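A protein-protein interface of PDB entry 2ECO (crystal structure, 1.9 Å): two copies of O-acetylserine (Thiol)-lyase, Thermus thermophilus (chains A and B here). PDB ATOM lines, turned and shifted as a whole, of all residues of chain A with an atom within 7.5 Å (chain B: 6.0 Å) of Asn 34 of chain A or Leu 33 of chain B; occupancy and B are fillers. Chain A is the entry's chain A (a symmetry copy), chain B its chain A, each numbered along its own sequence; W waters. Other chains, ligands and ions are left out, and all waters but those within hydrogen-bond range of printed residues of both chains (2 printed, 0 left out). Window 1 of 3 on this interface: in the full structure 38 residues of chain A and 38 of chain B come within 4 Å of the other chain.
Water W2 bridges the backbone carbonyl oxygen (O) of Pro 35 of chain A (2.8 Å) and the indole nitrogen (NE1) of Trp 293 of chain B (3.2 Å).
Water W1 bridges the backbone carbonyl oxygen (O) of Asn 34 of chain A (2.9 Å) and the indole nitrogen (NE1) of Trp 293 of chain B (3.4 Å).
Among the printed residues, pairs that only touch across the chains: Ala 6 of chain A with Pro 11 of chain B (3.8 Å), Pro 11 of chain A with Ala 6 of chain B (3.8 Å), Leu 33 of chain A with Leu 33 of chain B (3.97 Å), Leu 33 of chain A with Asn 34 of chain B (3.6 Å), Leu 33 of chain A with Pro 35 of chain B (3.7 Å), Asn 34 of chain A with Leu 33 of chain B (3.6 Å), Pro 35 of chain A with Leu 33 of chain B (3.7 Å), Gly 36 of chain A with Trp 293 of chain B (3.3 Å) and Gly 37 of chain A with Trp 293 of chain B (3.9 Å).
Of chain B, only Leu 33 comes within 4 Å of Asn 34 of chain A.
Leu 33 of chain B touches three residues of chain A.
No residue of chain A comes within 4 Å of Gly 32 of chain B.
Of the printed residues of chain B, Gly 36 of chain A touches Trp 293 (3.3 Å).
Of the printed residues of chain B, Pro 11 of chain A touches Ala 6 (3.8 Å).
Printed residues of chain B within 4 Å of Gly 37 of chain A: Trp 293.
Glu 31 of chain B touches none of the printed residues of chain A.
The nearest printed residue of chain A that does not touch Asn 34 of chain B is Gly 32 of chain A (6.7 Å).
O of Glu 31 of chain B is in hydrogen-bond range of ND2 of Asn 34 of chain B, at 2.9 Å.
The backbone carbonyl oxygen of Pro 11 of chain B is in hydrogen-bond range of the backbone NH of Leu 30 of chain B (3.0 Å).
N of Gly 36 of chain A lies within hydrogen-bond range of SD of Met 79 of chain A (3.5 Å).
The backbone NH (N) of Gly 8 of chain B sits at hydrogen-bond distance from the side-chain amide oxygen (OD1) of Asn 34 of chain B, 2.9 Å away.
The backbone carbonyl oxygen of Pro 11 of chain A is in hydrogen-bond range of the backbone NH of Leu 30 of chain A (3.0 Å).
N of Gly 36 of chain A is in hydrogen-bond range of OD2 of Asp 41 of chain A (2.5 Å).
Of the 13 printed residues of chain B, 6 touch a printed residue of chain A.
Printed residues of chain B that touch a printed residue of chain A: Ala 6, Pro 11, Leu 33, Asn 34, Pro 35 and Trp 293.
Hydrophobic or aromatic side chains of chain B within 4 Å of the printed part of chain A: Ala 6, Pro 11, Leu 33 and Trp 293.
Hydrophobic or aromatic side chains of chain A that line the printed part of chain B: Ala 6, Pro 11 and Leu 33.
Among the printed residues, 9 pairs touch across the chains.
Ala 6 of chain A touches Pro 11 of chain B, and with the chains exchanged Pro 11 of chain A touches Ala 6 of chain B.
Leu 33 of chain A touches its own counterpart, Leu 33 of chain B.
Leu 33 of chain A touches Asn 34 of chain B, and with the chains exchanged Asn 34 of chain A touches Leu 33 of chain B.
Leu 33 of chain A touches Pro 35 of chain B, and with the chains exchanged Pro 35 of chain A touches Leu 33 of chain B.
12 positions are printed for both chains.
Of the 9 pairs that touch across the chains among the printed residues, 7 have their exchanged pair printed and touching as well.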
ATOM      1  N   VAL A   3       0.540  -1.993   3.290  1.00  0.00           N
ATOM      2  CA  VAL A   3       0.734  -0.878   2.371  1.00  0.00           C
ATOM      3  C   VAL A   3       1.106   0.445   3.038  1.00  0.00           C
ATOM      4  O   VAL A   3       1.920   1.199   2.500  1.00  0.00           O
ATOM      5  CB  VAL A   3      -0.508  -0.671   1.464  1.00  0.00           C
ATOM      6  CG1 VAL A   3      -1.661  -0.098   2.267  1.00  0.00           C
ATOM      7  CG2 VAL A   3      -0.151   0.238   0.296  1.00  0.00           C
ATOM      8  N   ALA A   6       4.605   1.091   3.258  1.00  0.00           N
ATOM      9  CA  ALA A   6       5.320   1.327   2.006  1.00  0.00           C
ATOM     10  C   ALA A   6       5.342   2.807   1.632  1.00  0.00           C
ATOM     11  O   ALA A   6       5.852   3.184   0.572  1.00  0.00           O
ATOM     12  CB  ALA A   6       4.676   0.524   0.882  1.00  0.00           C
ATOM     13  N   ILE A   7       4.782   3.642   2.499  1.00  0.00           N
ATOM     14  CA  ILE A   7       4.737   5.081   2.263  1.00  0.00           C
ATOM     15  C   ILE A   7       6.043   5.753   2.686  1.00  0.00           C
ATOM     16  O   ILE A   7       6.631   5.391   3.706  1.00  0.00           O
ATOM     17  CB  ILE A   7       3.585   5.739   3.067  1.00  0.00           C
ATOM     18  CG1 ILE A   7       2.237   5.152   2.639  1.00  0.00           C
ATOM     19  CG2 ILE A   7       3.605   7.250   2.877  1.00  0.00           C
ATOM     20  CD1 ILE A   7       1.068   5.637   3.492  1.00  0.00           C
ATOM     21  N   GLY A   8       6.497   6.724   1.898  1.00  0.00           N
ATOM     22  CA  GLY A   8       7.703   7.455   2.249  1.00  0.00           C
ATOM     23  C   GLY A   8       9.019   6.976   1.669  1.00  0.00           C
ATOM     24  O   GLY A   8       9.054   6.114   0.784  1.00  0.00           O
ATOM     25  N   LYS A   9      10.107   7.552   2.174  1.00  0.00           N
ATOM     26  CA  LYS A   9      11.452   7.208   1.727  1.00  0.00           C
ATOM     27  C   LYS A   9      11.551   7.328   0.209  1.00  0.00           C
ATOM     28  O   LYS A   9      12.132   6.474  -0.454  1.00  0.00           O
ATOM     29  CB  LYS A   9      11.802   5.782   2.160  1.00  0.00           C
ATOM     30  CG  LYS A   9      11.729   5.548   3.660  1.00  0.00           C
ATOM     31  CD  LYS A   9      12.766   6.367   4.408  1.00  0.00           C
ATOM     32  CE  LYS A   9      12.793   5.999   5.886  1.00  0.00           C
ATOM     33  NZ  LYS A   9      13.860   6.736   6.629  1.00  0.00           N
ATOM     34  N   THR A  10      10.971   8.396  -0.326  1.00  0.00           N
ATOM     35  CA  THR A  10      10.978   8.645  -1.760  1.00  0.00           C
ATOM     36  C   THR A  10      12.315   9.244  -2.195  1.00  0.00           C
ATOM     37  O   THR A  10      12.984   9.930  -1.421  1.00  0.00           O
ATOM     38  CB  THR A  10       9.856   9.613  -2.146  1.00  0.00           C
ATOM     39  OG1 THR A  10       9.975  10.804  -1.359  1.00  0.00           O
ATOM     40  CG2 THR A  10       8.489   8.973  -1.902  1.00  0.00           C
ATOM     41  N   PRO A  11      12.709   9.005  -3.453  1.00  0.00           N
ATOM     42  CA  PRO A  11      13.977   9.525  -3.972  1.00  0.00           C
ATOM     43  C   PRO A  11      13.950  10.993  -4.384  1.00  0.00           C
ATOM     44  O   PRO A  11      12.885  11.584  -4.584  1.00  0.00           O
ATOM     45  CB  PRO A  11      14.256   8.606  -5.153  1.00  0.00           C
ATOM     46  CG  PRO A  11      12.880   8.376  -5.704  1.00  0.00           C
ATOM     47  CD  PRO A  11      12.040   8.150  -4.454  1.00  0.00           C
ATOM     48  N   LEU A  30      10.463  13.011  -5.501  1.00  0.00           N
ATOM     49  CA  LEU A  30       9.349  12.379  -6.205  1.00  0.00           C
ATOM     50  C   LEU A  30       8.323  11.685  -5.316  1.00  0.00           C
ATOM     51  O   LEU A  30       8.433  10.492  -5.043  1.00  0.00           O
ATOM     52  CB  LEU A  30       9.917  11.378  -7.220  1.00  0.00           C
ATOM     53  CG  LEU A  30      11.022  11.971  -8.110  1.00  0.00           C
ATOM     54  CD1 LEU A  30      11.620  10.889  -9.004  1.00  0.00           C
ATOM     55  CD2 LEU A  30      10.448  13.105  -8.948  1.00  0.00           C
ATOM     56  N   GLU A  31       7.310  12.430  -4.889  1.00  0.00           N
ATOM     57  CA  GLU A  31       6.277  11.869  -4.017  1.00  0.00           C
ATOM     58  C   GLU A  31       5.254  11.029  -4.763  1.00  0.00           C
ATOM     59  O   GLU A  31       4.380  10.406  -4.156  1.00  0.00           O
ATOM     60  CB  GLU A  31       5.587  12.995  -3.242  1.00  0.00           C
ATOM     61  CG  GLU A  31       6.489  13.592  -2.170  1.00  0.00           C
ATOM     62  CD  GLU A  31       6.838  12.583  -1.094  1.00  0.00           C
ATOM     63  OE1 GLU A  31       8.041  12.379  -0.826  1.00  0.00           O
ATOM     64  OE2 GLU A  31       5.905  11.992  -0.512  1.00  0.00           O
ATOM     65  N   GLY A  32       5.368  11.006  -6.084  1.00  0.00           N
ATOM     66  CA  GLY A  32       4.455  10.206  -6.875  1.00  0.00           C
ATOM     67  C   GLY A  32       4.783   8.731  -6.725  1.00  0.00           C
ATOM     68  O   GLY A  32       3.983   7.873  -7.090  1.00  0.00           O
ATOM     69  N   LEU A  33       5.957   8.429  -6.177  1.00  0.00           N
ATOM     70  CA  LEU A  33       6.359   7.039  -6.000  1.00  0.00           C
ATOM     71  C   LEU A  33       5.858   6.455  -4.683  1.00  0.00           C
ATOM     72  O   LEU A  33       6.522   5.638  -4.058  1.00  0.00           O
ATOM     73  CB  LEU A  33       7.887   6.905  -6.093  1.00  0.00           C
ATOM     74  CG  LEU A  33       8.485   7.357  -7.432  1.00  0.00           C
ATOM     75  CD1 LEU A  33       9.988   7.172  -7.410  1.00  0.00           C
ATOM     76  CD2 LEU A  33       7.868   6.557  -8.572  1.00  0.00           C
ATOM     77  N   ASN A  34       4.680   6.893  -4.262  1.00  0.00           N
ATOM     78  CA  ASN A  34       4.064   6.389  -3.045  1.00  0.00           C
ATOM     79  C   ASN A  34       2.972   5.422  -3.488  1.00  0.00           C
ATOM     80  O   ASN A  34       2.446   5.540  -4.596  1.00  0.00           O
ATOM     81  CB  ASN A  34       3.482   7.543  -2.221  1.00  0.00           C
ATOM     82  CG  ASN A  34       4.520   8.192  -1.325  1.00  0.00           C
ATOM     83  OD1 ASN A  34       5.181   7.513  -0.540  1.00  0.00           O
ATOM     84  ND2 ASN A  34       4.668   9.507  -1.435  1.00  0.00           N
ATOM     85  N   PRO A  35       2.617   4.449  -2.632  1.00  0.00           N
ATOM     86  CA  PRO A  35       1.583   3.471  -2.985  1.00  0.00           C
ATOM     87  C   PRO A  35       0.242   4.072  -3.393  1.00  0.00           C
ATOM     88  O   PRO A  35      -0.502   3.468  -4.164  1.00  0.00           O
ATOM     89  CB  PRO A  35       1.489   2.595  -1.734  1.00  0.00           C
ATOM     90  CG  PRO A  35       1.891   3.531  -0.631  1.00  0.00           C
ATOM     91  CD  PRO A  35       3.060   4.267  -1.238  1.00  0.00           C
ATOM     92  N   GLY A  36      -0.059   5.255  -2.869  1.00  0.00           N
ATOM     93  CA  GLY A  36      -1.308   5.915  -3.200  1.00  0.00           C
ATOM     94  C   GLY A  36      -1.132   6.832  -4.396  1.00  0.00           C
ATOM     95  O   GLY A  36      -2.081   7.470  -4.844  1.00  0.00           O
ATOM     96  N   GLY A  37       0.099   6.907  -4.896  1.00  0.00           N
ATOM     97  CA  GLY A  37       0.392   7.732  -6.055  1.00  0.00           C
ATOM     98  C   GLY A  37       0.703   9.197  -5.807  1.00  0.00           C
ATOM     99  O   GLY A  37       0.900   9.945  -6.766  1.00  0.00           O
ATOM    100  N   SER A  38       0.758   9.629  -4.548  1.00  0.00           N
ATOM    101  CA  SER A  38       1.050  11.035  -4.281  1.00  0.00           C
ATOM    102  C   SER A  38       1.530  11.304  -2.866  1.00  0.00           C
ATOM    103  O   SER A  38       1.493  10.433  -1.998  1.00  0.00           O
ATOM    104  CB  SER A  38      -0.192  11.896  -4.519  1.00  0.00           C
ATOM    105  OG  SER A  38      -1.032  11.891  -3.370  1.00  0.00           O
ATOM    106  N   ILE A  39       1.958  12.541  -2.647  1.00  0.00           N
ATOM    107  CA  ILE A  39       2.439  12.979  -1.346  1.00  0.00           C
ATOM    108  C   ILE A  39       1.346  12.876  -0.277  1.00  0.00           C
ATOM    109  O   ILE A  39       1.652  12.791   0.913  1.00  0.00           O
ATOM    110  CB  ILE A  39       2.946  14.439  -1.428  1.00  0.00           C
ATOM    111  CG1 ILE A  39       3.605  14.850  -0.112  1.00  0.00           C
ATOM    112  CG2 ILE A  39       1.797  15.369  -1.789  1.00  0.00           C
ATOM    113  CD1 ILE A  39       4.245  16.227  -0.174  1.00  0.00           C
ATOM    114  N   LYS A  40       0.079  12.879  -0.693  1.00  0.00           N
ATOM    115  CA  LYS A  40      -1.030  12.799   0.263  1.00  0.00           C
ATOM    116  C   LYS A  40      -1.075  11.499   1.055  1.00  0.00           C
ATOM    117  O   LYS A  40      -1.813  11.397   2.031  1.00  0.00           O
ATOM    118  CB  LYS A  40      -2.377  12.995  -0.432  1.00  0.00           C
ATOM    119  CG  LYS A  40      -2.636  14.398  -0.927  1.00  0.00           C
ATOM    120  CD  LYS A  40      -2.506  15.439   0.188  1.00  0.00           C
ATOM    121  CE  LYS A  40      -3.250  16.728  -0.179  1.00  0.00           C
ATOM    122  NZ  LYS A  40      -2.918  17.111  -1.573  1.00  0.00           N
ATOM    123  N   ASP A  41      -0.313  10.498   0.630  1.00  0.00           N
ATOM    124  CA  ASP A  41      -0.268   9.236   1.366  1.00  0.00           C
ATOM    125  C   ASP A  41       0.188   9.526   2.800  1.00  0.00           C
ATOM    126  O   ASP A  41      -0.288   8.911   3.756  1.00  0.00           O
ATOM    127  CB  ASP A  41       0.741   8.277   0.731  1.00  0.00           C
ATOM    128  CG  ASP A  41       0.173   7.511  -0.447  1.00  0.00           C
ATOM    129  OD1 ASP A  41      -0.882   7.910  -0.981  1.00  0.00           O
ATOM    130  OD2 ASP A  41       0.804   6.508  -0.842  1.00  0.00           O
ATOM    131  N   ARG A  42       1.115  10.469   2.934  1.00  0.00           N
ATOM    132  CA  ARG A  42       1.666  10.825   4.241  1.00  0.00           C
ATOM    133  C   ARG A  42       0.637  11.428   5.207  1.00  0.00           C
ATOM    134  O   ARG A  42       0.432  10.903   6.305  1.00  0.00           O
ATOM    135  CB  ARG A  42       2.865  11.771   4.061  1.00  0.00           C
ATOM    136  CG  ARG A  42       4.025  11.168   3.241  1.00  0.00           C
ATOM    137  CD  ARG A  42       5.192  12.151   3.113  1.00  0.00           C
ATOM    138  NE  ARG A  42       6.257  11.697   2.212  1.00  0.00           N
ATOM    139  CZ  ARG A  42       7.392  11.113   2.598  1.00  0.00           C
ATOM    140  NH1 ARG A  42       7.634  10.893   3.884  1.00  0.00           N
ATOM    141  NH2 ARG A  42       8.303  10.771   1.693  1.00  0.00           N
ATOM    142  N   MET A  79      -7.047   4.331   0.360  1.00  0.00           N
ATOM    143  CA  MET A  79      -6.054   3.273   0.472  1.00  0.00           C
ATOM    144  C   MET A  79      -5.885   2.818   1.918  1.00  0.00           C
ATOM    145  O   MET A  79      -5.909   1.620   2.207  1.00  0.00           O
ATOM    146  CB  MET A  79      -4.712   3.763  -0.072  1.00  0.00           C
ATOM    147  CG  MET A  79      -3.573   2.770   0.088  1.00  0.00           C
ATOM    148  SD  MET A  79      -2.048   3.405  -0.638  1.00  0.00           S
ATOM    149  CE  MET A  79      -1.537   4.581   0.621  1.00  0.00           C
ATOM    150  N   GLU A 158      13.775  13.309   5.576  1.00  0.00           N
ATOM    151  CA  GLU A 158      14.213  12.620   4.365  1.00  0.00           C
ATOM    152  C   GLU A 158      14.936  13.555   3.406  1.00  0.00           C
ATOM    153  O   GLU A 158      16.025  13.245   2.918  1.00  0.00           O
ATOM    154  CB  GLU A 158      13.013  12.003   3.643  1.00  0.00           C
ATOM    155  CG  GLU A 158      12.498  10.715   4.257  1.00  0.00           C
ATOM    156  CD  GLU A 158      11.238  10.215   3.571  1.00  0.00           C
ATOM    157  OE1 GLU A 158      11.096  10.437   2.349  1.00  0.00           O
ATOM    158  OE2 GLU A 158      10.401   9.589   4.252  1.00  0.00           O
ATOM    159  N   SER A 288       7.805  17.123  -5.931  1.00  0.00           N
ATOM    160  CA  SER A 288       6.840  16.790  -6.973  1.00  0.00           C
ATOM    161  C   SER A 288       5.738  16.029  -6.241  1.00  0.00           C
ATOM    162  O   SER A 288       5.950  14.911  -5.785  1.00  0.00           O
ATOM    163  CB  SER A 288       7.467  15.879  -8.030  1.00  0.00           C
ATOM    164  OG  SER A 288       6.469  15.350  -8.896  1.00  0.00           O
ATOM    165  N   PRO A 289       4.550  16.633  -6.113  1.00  0.00           N
ATOM    166  CA  PRO A 289       3.420  16.002  -5.421  1.00  0.00           C
ATOM    167  C   PRO A 289       2.966  14.659  -5.993  1.00  0.00           C
ATOM    168  O   PRO A 289       2.660  13.740  -5.241  1.00  0.00           O
ATOM    169  CB  PRO A 289       2.336  17.069  -5.497  1.00  0.00           C
ATOM    170  CG  PRO A 289       3.139  18.356  -5.505  1.00  0.00           C
ATOM    171  CD  PRO A 289       4.230  18.023  -6.483  1.00  0.00           C
ATOM    172  N   ALA B   6      16.567   6.193  -9.561  1.00  0.00           N
ATOM    173  CA  ALA B   6      15.401   6.051  -8.694  1.00  0.00           C
ATOM    174  C   ALA B   6      14.694   4.714  -8.901  1.00  0.00           C
ATOM    175  O   ALA B   6      13.652   4.448  -8.293  1.00  0.00           O
ATOM    176  CB  ALA B   6      14.424   7.192  -8.947  1.00  0.00           C
ATOM    177  N   GLY B   8      14.177   0.664  -8.626  1.00  0.00           N
ATOM    178  CA  GLY B   8      14.502  -0.387  -7.675  1.00  0.00           C
ATOM    179  C   GLY B   8      14.231  -0.126  -6.206  1.00  0.00           C
ATOM    180  O   GLY B   8      13.588   0.863  -5.838  1.00  0.00           O
ATOM    181  N   THR B  10      12.233  -1.536  -4.250  1.00  0.00           N
ATOM    182  CA  THR B  10      10.795  -1.487  -4.033  1.00  0.00           C
ATOM    183  C   THR B  10      10.412  -2.285  -2.787  1.00  0.00           C
ATOM    184  O   THR B  10      11.084  -3.251  -2.422  1.00  0.00           O
ATOM    185  CB  THR B  10      10.046  -2.064  -5.237  1.00  0.00           C
ATOM    186  OG1 THR B  10      10.538  -3.382  -5.505  1.00  0.00           O
ATOM    187  CG2 THR B  10      10.252  -1.182  -6.469  1.00  0.00           C
ATOM    188  N   PRO B  11       9.310  -1.898  -2.131  1.00  0.00           N
ATOM    189  CA  PRO B  11       8.855  -2.588  -0.920  1.00  0.00           C
ATOM    190  C   PRO B  11       8.108  -3.894  -1.167  1.00  0.00           C
ATOM    191  O   PRO B  11       7.634  -4.164  -2.274  1.00  0.00           O
ATOM    192  CB  PRO B  11       7.973  -1.543  -0.253  1.00  0.00           C
ATOM    193  CG  PRO B  11       7.315  -0.888  -1.432  1.00  0.00           C
ATOM    194  CD  PRO B  11       8.460  -0.726  -2.422  1.00  0.00           C
ATOM    195  N   LEU B  30       6.095  -4.765  -4.726  1.00  0.00           N
ATOM    196  CA  LEU B  30       5.418  -3.758  -5.543  1.00  0.00           C
ATOM    197  C   LEU B  30       6.303  -3.035  -6.553  1.00  0.00           C
ATOM    198  O   LEU B  30       6.862  -1.981  -6.258  1.00  0.00           O
ATOM    199  CB  LEU B  30       4.753  -2.737  -4.611  1.00  0.00           C
ATOM    200  CG  LEU B  30       3.902  -3.383  -3.505  1.00  0.00           C
ATOM    201  CD1 LEU B  30       3.377  -2.316  -2.549  1.00  0.00           C
ATOM    202  CD2 LEU B  30       2.752  -4.157  -4.133  1.00  0.00           C
ATOM    203  N   GLU B  31       6.404  -3.589  -7.756  1.00  0.00           N
ATOM    204  CA  GLU B  31       7.239  -2.987  -8.796  1.00  0.00           C
ATOM    205  C   GLU B  31       6.583  -1.796  -9.476  1.00  0.00           C
ATOM    206  O   GLU B  31       7.199  -1.119 -10.303  1.00  0.00           O
ATOM    207  CB  GLU B  31       7.626  -4.050  -9.827  1.00  0.00           C
ATOM    208  CG  GLU B  31       8.637  -5.046  -9.273  1.00  0.00           C
ATOM    209  CD  GLU B  31       9.957  -4.386  -8.931  1.00  0.00           C
ATOM    210  OE1 GLU B  31      10.423  -4.531  -7.780  1.00  0.00           O
ATOM    211  OE2 GLU B  31      10.534  -3.720  -9.815  1.00  0.00           O
ATOM    212  N   GLY B  32       5.332  -1.536  -9.121  1.00  0.00           N
ATOM    213  CA  GLY B  32       4.639  -0.401  -9.696  1.00  0.00           C
ATOM    214  C   GLY B  32       5.176   0.894  -9.111  1.00  0.00           C
ATOM    215  O   GLY B  32       4.921   1.972  -9.642  1.00  0.00           O
ATOM    216  N   LEU B  33       5.930   0.793  -8.020  1.00  0.00           N
ATOM    217  CA  LEU B  33       6.482   1.984  -7.386  1.00  0.00           C
ATOM    218  C   LEU B  33       7.821   2.393  -7.990  1.00  0.00           C
ATOM    219  O   LEU B  33       8.704   2.887  -7.300  1.00  0.00           O
ATOM    220  CB  LEU B  33       6.626   1.769  -5.872  1.00  0.00           C
ATOM    221  CG  LEU B  33       5.310   1.467  -5.143  1.00  0.00           C
ATOM    222  CD1 LEU B  33       5.574   1.283  -3.663  1.00  0.00           C
ATOM    223  CD2 LEU B  33       4.320   2.602  -5.369  1.00  0.00           C
ATOM    224  N   ASN B  34       7.967   2.170  -9.289  1.00  0.00           N
ATOM    225  CA  ASN B  34       9.176   2.551 -10.002  1.00  0.00           C
ATOM    226  C   ASN B  34       8.834   3.817 -10.778  1.00  0.00           C
ATOM    227  O   ASN B  34       7.670   4.052 -11.106  1.00  0.00           O
ATOM    228  CB  ASN B  34       9.620   1.425 -10.943  1.00  0.00           C
ATOM    229  CG  ASN B  34      10.466   0.383 -10.237  1.00  0.00           C
ATOM    230  OD1 ASN B  34      11.469   0.715  -9.607  1.00  0.00           O
ATOM    231  ND2 ASN B  34      10.069  -0.880 -10.339  1.00  0.00           N
ATOM    232  N   PRO B  35       9.841   4.653 -11.080  1.00  0.00           N
ATOM    233  CA  PRO B  35       9.595   5.899 -11.814  1.00  0.00           C
ATOM    234  C   PRO B  35       8.884   5.727 -13.152  1.00  0.00           C
ATOM    235  O   PRO B  35       8.185   6.632 -13.607  1.00  0.00           O
ATOM    236  CB  PRO B  35      10.994   6.502 -11.956  1.00  0.00           C
ATOM    237  CG  PRO B  35      11.888   5.296 -11.957  1.00  0.00           C
ATOM    238  CD  PRO B  35      11.284   4.442 -10.869  1.00  0.00           C
ATOM    239  N   GLY B  37       6.747   3.367 -13.587  1.00  0.00           N
ATOM    240  CA  GLY B  37       5.475   2.746 -13.259  1.00  0.00           C
ATOM    241  C   GLY B  37       5.409   1.230 -13.299  1.00  0.00           C
ATOM    242  O   GLY B  37       4.335   0.665 -13.086  1.00  0.00           O
ATOM    243  N   SER B  38       6.526   0.554 -13.562  1.00  0.00           N
ATOM    244  CA  SER B  38       6.489  -0.906 -13.612  1.00  0.00           C
ATOM    245  C   SER B  38       7.852  -1.560 -13.461  1.00  0.00           C
ATOM    246  O   SER B  38       8.889  -0.897 -13.479  1.00  0.00           O
ATOM    247  CB  SER B  38       5.892  -1.383 -14.937  1.00  0.00           C
ATOM    248  OG  SER B  38       6.888  -1.410 -15.953  1.00  0.00           O
ATOM    249  N   TRP B 293      -3.121   2.051 -12.026  1.00  0.00           N
ATOM    250  CA  TRP B 293      -3.227   3.368 -12.666  1.00  0.00           C
ATOM    251  C   TRP B 293      -3.441   3.407 -14.182  1.00  0.00           C
ATOM    252  O   TRP B 293      -4.130   4.297 -14.686  1.00  0.00           O
ATOM    253  CB  TRP B 293      -2.004   4.224 -12.312  1.00  0.00           C
ATOM    254  CG  TRP B 293      -1.717   4.248 -10.841  1.00  0.00           C
ATOM    255  CD1 TRP B 293      -0.769   3.522 -10.180  1.00  0.00           C
ATOM    256  CD2 TRP B 293      -2.443   4.969  -9.837  1.00  0.00           C
ATOM    257  NE1 TRP B 293      -0.863   3.741  -8.825  1.00  0.00           N
ATOM    258  CE2 TRP B 293      -1.882   4.624  -8.587  1.00  0.00           C
ATOM    259  CE3 TRP B 293      -3.518   5.869  -9.872  1.00  0.00           C
ATOM    260  CZ2 TRP B 293      -2.361   5.149  -7.379  1.00  0.00           C
ATOM    261  CZ3 TRP B 293      -3.993   6.391  -8.670  1.00  0.00           C
ATOM    262  CH2 TRP B 293      -3.413   6.027  -7.442  1.00  0.00           C
HETATM  263  O   HOH W   1       2.070   4.491  -7.308  1.00  0.00           O
HETATM  264  O   HOH W   2       0.334   2.054  -6.388  1.00  0.00           O
